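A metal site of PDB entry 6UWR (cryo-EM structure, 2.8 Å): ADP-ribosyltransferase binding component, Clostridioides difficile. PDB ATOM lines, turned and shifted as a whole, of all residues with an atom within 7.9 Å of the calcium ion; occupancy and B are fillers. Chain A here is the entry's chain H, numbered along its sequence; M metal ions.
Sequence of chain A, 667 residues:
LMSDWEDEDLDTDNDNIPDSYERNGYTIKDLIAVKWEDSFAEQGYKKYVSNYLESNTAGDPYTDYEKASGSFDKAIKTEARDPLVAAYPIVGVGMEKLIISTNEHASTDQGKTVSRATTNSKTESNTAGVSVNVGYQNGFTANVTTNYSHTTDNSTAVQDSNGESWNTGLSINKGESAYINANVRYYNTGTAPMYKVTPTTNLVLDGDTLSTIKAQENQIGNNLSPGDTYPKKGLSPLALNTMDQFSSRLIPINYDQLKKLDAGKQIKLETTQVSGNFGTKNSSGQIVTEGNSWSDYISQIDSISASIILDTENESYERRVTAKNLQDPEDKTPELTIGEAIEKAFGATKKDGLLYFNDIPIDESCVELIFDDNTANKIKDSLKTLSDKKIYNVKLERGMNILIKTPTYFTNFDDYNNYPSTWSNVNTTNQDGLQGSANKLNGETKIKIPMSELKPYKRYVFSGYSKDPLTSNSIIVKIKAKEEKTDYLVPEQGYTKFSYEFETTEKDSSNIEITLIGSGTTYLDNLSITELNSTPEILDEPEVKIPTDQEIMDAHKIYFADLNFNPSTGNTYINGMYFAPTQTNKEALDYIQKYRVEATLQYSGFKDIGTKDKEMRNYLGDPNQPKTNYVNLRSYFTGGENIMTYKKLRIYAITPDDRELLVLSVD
OD2 of Asp 525 sits close to O of Gly 433 (2.6 Å). The side-chain amide oxygen (OD1) of Asn 412 is in hydrogen-bond range of the backbone NH (N) of Asp 415 (3.5 Å). O of Asp 432 sits close to O of Ser 437, at 2.7 Å.
Within 4 Å of the calcium ion: Asn 412, Asp 414, Gln 435, Ser 437 and Asp 525. Along chain A the residues within 4 Å of the calcium ion span positions 412 to 525. The nearest printed residue that does not touch the calcium ion is Gly 436 (4.1 Å).
The calcium ion is bound by the side-chain carboxylate (OD2) of Asp 525, 2.3 Å away. OD2 of Asp 414 binds the calcium ion. O of Gln 435 binds the calcium ion (2.4 Å). The backbone carbonyl oxygen (O) of Asn 412 binds the calcium ion (2.4 Å). The side-chain carboxylate (OD1) of Asp 414 binds the calcium ion. The calcium ion is bound by the backbone carbonyl oxygen (O) of Ser 437. The calcium ion has six donor atoms within binding distance. Slightly farther from the calcium ion lies the side-chain carboxylate (OD1) of Asp 525 (3.0 Å).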
ATOM      1  N   PHE A 410      19.144 -10.249 -14.385  1.00  0.00           N
ATOM      2  CA  PHE A 410      20.083  -9.140 -14.287  1.00  0.00           C
ATOM      3  C   PHE A 410      21.496  -9.673 -14.184  1.00  0.00           C
ATOM      4  O   PHE A 410      21.727 -10.718 -13.565  1.00  0.00           O
ATOM      5  CB  PHE A 410      19.748  -8.272 -13.066  1.00  0.00           C
ATOM      6  CG  PHE A 410      20.669  -7.112 -12.875  1.00  0.00           C
ATOM      7  CD1 PHE A 410      20.561  -5.979 -13.652  1.00  0.00           C
ATOM      8  CD2 PHE A 410      21.646  -7.147 -11.901  1.00  0.00           C
ATOM      9  CE1 PHE A 410      21.392  -4.921 -13.472  1.00  0.00           C
ATOM     10  CE2 PHE A 410      22.483  -6.086 -11.714  1.00  0.00           C
ATOM     11  CZ  PHE A 410      22.360  -4.973 -12.510  1.00  0.00           C
ATOM     12  N   THR A 411      22.431  -8.961 -14.813  1.00  0.00           N
ATOM     13  CA  THR A 411      23.862  -9.228 -14.663  1.00  0.00           C
ATOM     14  C   THR A 411      24.612  -7.912 -14.633  1.00  0.00           C
ATOM     15  O   THR A 411      24.398  -7.052 -15.488  1.00  0.00           O
ATOM     16  CB  THR A 411      24.427 -10.080 -15.811  1.00  0.00           C
ATOM     17  OG1 THR A 411      23.775  -9.740 -17.038  1.00  0.00           O
ATOM     18  CG2 THR A 411      24.244 -11.551 -15.519  1.00  0.00           C
ATOM     19  N   ASN A 412      25.488  -7.767 -13.647  1.00  0.00           N
ATOM     20  CA  ASN A 412      26.457  -6.679 -13.609  1.00  0.00           C
ATOM     21  C   ASN A 412      27.823  -7.129 -14.071  1.00  0.00           C
ATOM     22  O   ASN A 412      28.770  -6.350 -14.009  1.00  0.00           O
ATOM     23  CB  ASN A 412      26.537  -6.104 -12.203  1.00  0.00           C
ATOM     24  CG  ASN A 412      26.762  -7.178 -11.157  1.00  0.00           C
ATOM     25  OD1 ASN A 412      26.726  -8.366 -11.467  1.00  0.00           O
ATOM     26  ND2 ASN A 412      26.996  -6.767  -9.920  1.00  0.00           N
ATOM     27  N   PHE A 413      27.941  -8.385 -14.500  1.00  0.00           N
ATOM     28  CA  PHE A 413      29.195  -8.995 -14.936  1.00  0.00           C
ATOM     29  C   PHE A 413      30.240  -9.024 -13.824  1.00  0.00           C
ATOM     30  O   PHE A 413      31.415  -9.312 -14.098  1.00  0.00           O
ATOM     31  CB  PHE A 413      29.764  -8.280 -16.163  1.00  0.00           C
ATOM     32  CG  PHE A 413      28.855  -8.308 -17.353  1.00  0.00           C
ATOM     33  CD1 PHE A 413      28.520  -9.502 -17.955  1.00  0.00           C
ATOM     34  CD2 PHE A 413      28.361  -7.135 -17.889  1.00  0.00           C
ATOM     35  CE1 PHE A 413      27.691  -9.538 -19.055  1.00  0.00           C
ATOM     36  CE2 PHE A 413      27.535  -7.159 -18.984  1.00  0.00           C
ATOM     37  CZ  PHE A 413      27.204  -8.359 -19.570  1.00  0.00           C
ATOM     38  N   ASP A 414      29.871  -8.743 -12.581  1.00  0.00           N
ATOM     39  CA  ASP A 414      30.842  -8.739 -11.491  1.00  0.00           C
ATOM     40  C   ASP A 414      30.585  -9.847 -10.484  1.00  0.00           C
ATOM     41  O   ASP A 414      31.454 -10.711 -10.292  1.00  0.00           O
ATOM     42  CB  ASP A 414      30.855  -7.384 -10.785  1.00  0.00           C
ATOM     43  CG  ASP A 414      30.867  -6.213 -11.748  1.00  0.00           C
ATOM     44  OD1 ASP A 414      31.285  -6.406 -12.909  1.00  0.00           O
ATOM     45  OD2 ASP A 414      30.459  -5.110 -11.353  1.00  0.00           O
ATOM     46  N   ASP A 415      29.431  -9.869  -9.833  1.00  0.00           N
ATOM     47  CA  ASP A 415      29.136 -10.898  -8.847  1.00  0.00           C
ATOM     48  C   ASP A 415      27.722 -11.439  -8.918  1.00  0.00           C
ATOM     49  O   ASP A 415      27.469 -12.512  -8.353  1.00  0.00           O
ATOM     50  CB  ASP A 415      29.408 -10.386  -7.423  1.00  0.00           C
ATOM     51  CG  ASP A 415      28.175  -9.802  -6.745  1.00  0.00           C
ATOM     52  OD1 ASP A 415      27.347 -10.577  -6.223  1.00  0.00           O
ATOM     53  OD2 ASP A 415      28.035  -8.561  -6.738  1.00  0.00           O
ATOM     54  N   GLN A 431      37.925  -3.124 -15.993  1.00  0.00           N
ATOM     55  CA  GLN A 431      37.643  -2.240 -14.872  1.00  0.00           C
ATOM     56  C   GLN A 431      36.736  -1.074 -15.248  1.00  0.00           C
ATOM     57  O   GLN A 431      36.942   0.040 -14.747  1.00  0.00           O
ATOM     58  CB  GLN A 431      38.936  -1.721 -14.260  1.00  0.00           C
ATOM     59  CG  GLN A 431      38.913  -1.767 -12.737  1.00  0.00           C
ATOM     60  CD  GLN A 431      38.832  -3.180 -12.206  1.00  0.00           C
ATOM     61  OE1 GLN A 431      39.621  -4.053 -12.589  1.00  0.00           O
ATOM     62  NE2 GLN A 431      37.862  -3.430 -11.340  1.00  0.00           N
ATOM     63  N   ASP A 432      35.776  -1.289 -16.133  1.00  0.00           N
ATOM     64  CA  ASP A 432      34.758  -0.302 -16.473  1.00  0.00           C
ATOM     65  C   ASP A 432      33.379  -0.860 -16.145  1.00  0.00           C
ATOM     66  O   ASP A 432      33.242  -1.939 -15.567  1.00  0.00           O
ATOM     67  CB  ASP A 432      34.881   0.110 -17.932  1.00  0.00           C
ATOM     68  CG  ASP A 432      36.324   0.215 -18.382  1.00  0.00           C
ATOM     69  OD1 ASP A 432      37.120   0.860 -17.661  1.00  0.00           O
ATOM     70  OD2 ASP A 432      36.660  -0.364 -19.438  1.00  0.00           O
ATOM     71  N   GLY A 433      32.333  -0.131 -16.525  1.00  0.00           N
ATOM     72  CA  GLY A 433      30.969  -0.560 -16.310  1.00  0.00           C
ATOM     73  C   GLY A 433      30.211   0.219 -15.267  1.00  0.00           C
ATOM     74  O   GLY A 433      29.173  -0.256 -14.800  1.00  0.00           O
ATOM     75  N   LEU A 434      30.715   1.381 -14.860  1.00  0.00           N
ATOM     76  CA  LEU A 434      30.213   2.205 -13.769  1.00  0.00           C
ATOM     77  C   LEU A 434      30.540   1.536 -12.436  1.00  0.00           C
ATOM     78  O   LEU A 434      30.492   2.174 -11.382  1.00  0.00           O
ATOM     79  CB  LEU A 434      28.697   2.403 -13.862  1.00  0.00           C
ATOM     80  CG  LEU A 434      28.039   2.931 -15.125  1.00  0.00           C
ATOM     81  CD1 LEU A 434      26.753   2.176 -15.343  1.00  0.00           C
ATOM     82  CD2 LEU A 434      27.766   4.413 -14.995  1.00  0.00           C
ATOM     83  N   GLN A 435      30.915   0.260 -12.491  1.00  0.00           N
ATOM     84  CA  GLN A 435      31.313  -0.518 -11.325  1.00  0.00           C
ATOM     85  C   GLN A 435      31.824  -1.883 -11.776  1.00  0.00           C
ATOM     86  O   GLN A 435      31.156  -2.565 -12.563  1.00  0.00           O
ATOM     87  CB  GLN A 435      30.138  -0.668 -10.355  1.00  0.00           C
ATOM     88  CG  GLN A 435      28.816  -0.979 -11.021  1.00  0.00           C
ATOM     89  CD  GLN A 435      27.685  -0.140 -10.484  1.00  0.00           C
ATOM     90  OE1 GLN A 435      27.892   0.968 -10.026  1.00  0.00           O
ATOM     91  NE2 GLN A 435      26.474  -0.676 -10.553  1.00  0.00           N
ATOM     92  N   GLY A 436      32.986  -2.288 -11.295  1.00  0.00           N
ATOM     93  CA  GLY A 436      33.462  -3.634 -11.550  1.00  0.00           C
ATOM     94  C   GLY A 436      33.869  -3.825 -12.992  1.00  0.00           C
ATOM     95  O   GLY A 436      34.674  -3.072 -13.525  1.00  0.00           O
ATOM     96  N   SER A 437      33.302  -4.855 -13.629  1.00  0.00           N
ATOM     97  CA  SER A 437      33.684  -5.288 -14.963  1.00  0.00           C
ATOM     98  C   SER A 437      32.646  -4.851 -15.994  1.00  0.00           C
ATOM     99  O   SER A 437      31.661  -4.176 -15.676  1.00  0.00           O
ATOM    100  CB  SER A 437      33.859  -6.810 -14.969  1.00  0.00           C
ATOM    101  OG  SER A 437      34.493  -7.239 -13.780  1.00  0.00           O
ATOM    102  N   ALA A 438      32.859  -5.239 -17.242  1.00  0.00           N
ATOM    103  CA  ALA A 438      31.994  -4.876 -18.347  1.00  0.00           C
ATOM    104  C   ALA A 438      32.065  -5.993 -19.385  1.00  0.00           C
ATOM    105  O   ALA A 438      32.445  -7.118 -19.076  1.00  0.00           O
ATOM    106  CB  ALA A 438      32.385  -3.498 -18.908  1.00  0.00           C
ATOM    107  N   ASN A 439      31.649  -5.691 -20.617  1.00  0.00           N
ATOM    108  CA  ASN A 439      31.722  -6.643 -21.715  1.00  0.00           C
ATOM    109  C   ASN A 439      32.539  -6.056 -22.868  1.00  0.00           C
ATOM    110  O   ASN A 439      32.705  -4.843 -22.979  1.00  0.00           O
ATOM    111  CB  ASN A 439      30.328  -7.039 -22.200  1.00  0.00           C
ATOM    112  CG  ASN A 439      30.043  -8.503 -22.008  1.00  0.00           C
ATOM    113  OD1 ASN A 439      30.489  -9.121 -21.042  1.00  0.00           O
ATOM    114  ND2 ASN A 439      29.306  -9.095 -22.941  1.00  0.00           N
ATOM    115  N   TYR A 495      28.971   6.873 -20.156  1.00  0.00           N
ATOM    116  CA  TYR A 495      28.001   5.789 -20.038  1.00  0.00           C
ATOM    117  C   TYR A 495      26.579   6.326 -20.149  1.00  0.00           C
ATOM    118  O   TYR A 495      26.249   7.371 -19.577  1.00  0.00           O
ATOM    119  CB  TYR A 495      28.175   5.047 -18.715  1.00  0.00           C
ATOM    120  CG  TYR A 495      28.859   3.714 -18.862  1.00  0.00           C
ATOM    121  CD1 TYR A 495      28.179   2.629 -19.368  1.00  0.00           C
ATOM    122  CD2 TYR A 495      30.170   3.545 -18.497  1.00  0.00           C
ATOM    123  CE1 TYR A 495      28.788   1.409 -19.507  1.00  0.00           C
ATOM    124  CE2 TYR A 495      30.796   2.322 -18.634  1.00  0.00           C
ATOM    125  CZ  TYR A 495      30.098   1.263 -19.137  1.00  0.00           C
ATOM    126  OH  TYR A 495      30.698   0.049 -19.284  1.00  0.00           O
ATOM    127  N   LEU A 524      29.712  -3.058 -22.270  1.00  0.00           N
ATOM    128  CA  LEU A 524      28.345  -3.297 -21.818  1.00  0.00           C
ATOM    129  C   LEU A 524      28.328  -3.687 -20.350  1.00  0.00           C
ATOM    130  O   LEU A 524      29.148  -4.496 -19.911  1.00  0.00           O
ATOM    131  CB  LEU A 524      27.678  -4.406 -22.627  1.00  0.00           C
ATOM    132  CG  LEU A 524      27.470  -4.141 -24.115  1.00  0.00           C
ATOM    133  CD1 LEU A 524      26.649  -5.275 -24.699  1.00  0.00           C
ATOM    134  CD2 LEU A 524      26.778  -2.819 -24.332  1.00  0.00           C
ATOM    135  N   ASP A 525      27.405  -3.098 -19.594  1.00  0.00           N
ATOM    136  CA  ASP A 525      27.237  -3.474 -18.200  1.00  0.00           C
ATOM    137  C   ASP A 525      25.778  -3.309 -17.791  1.00  0.00           C
ATOM    138  O   ASP A 525      25.018  -2.559 -18.398  1.00  0.00           O
ATOM    139  CB  ASP A 525      28.124  -2.648 -17.266  1.00  0.00           C
ATOM    140  CG  ASP A 525      28.571  -3.431 -16.054  1.00  0.00           C
ATOM    141  OD1 ASP A 525      28.309  -4.652 -16.025  1.00  0.00           O
ATOM    142  OD2 ASP A 525      29.175  -2.851 -15.139  1.00  0.00           O
ATOM    143  N   ASN A 526      25.415  -4.049 -16.738  1.00  0.00           N
ATOM    144  CA  ASN A 526      24.099  -3.928 -16.087  1.00  0.00           C
ATOM    145  C   ASN A 526      22.958  -4.249 -17.044  1.00  0.00           C
ATOM    146  O   ASN A 526      22.046  -3.448 -17.250  1.00  0.00           O
ATOM    147  CB  ASN A 526      23.924  -2.543 -15.473  1.00  0.00           C
ATOM    148  CG  ASN A 526      24.767  -2.346 -14.225  1.00  0.00           C
ATOM    149  OD1 ASN A 526      25.352  -3.289 -13.705  1.00  0.00           O
ATOM    150  ND2 ASN A 526      24.828  -1.118 -13.741  1.00  0.00           N
HETATM  151 CA    CA M   1      29.831  -4.302 -13.473  1.00  0.00          CA
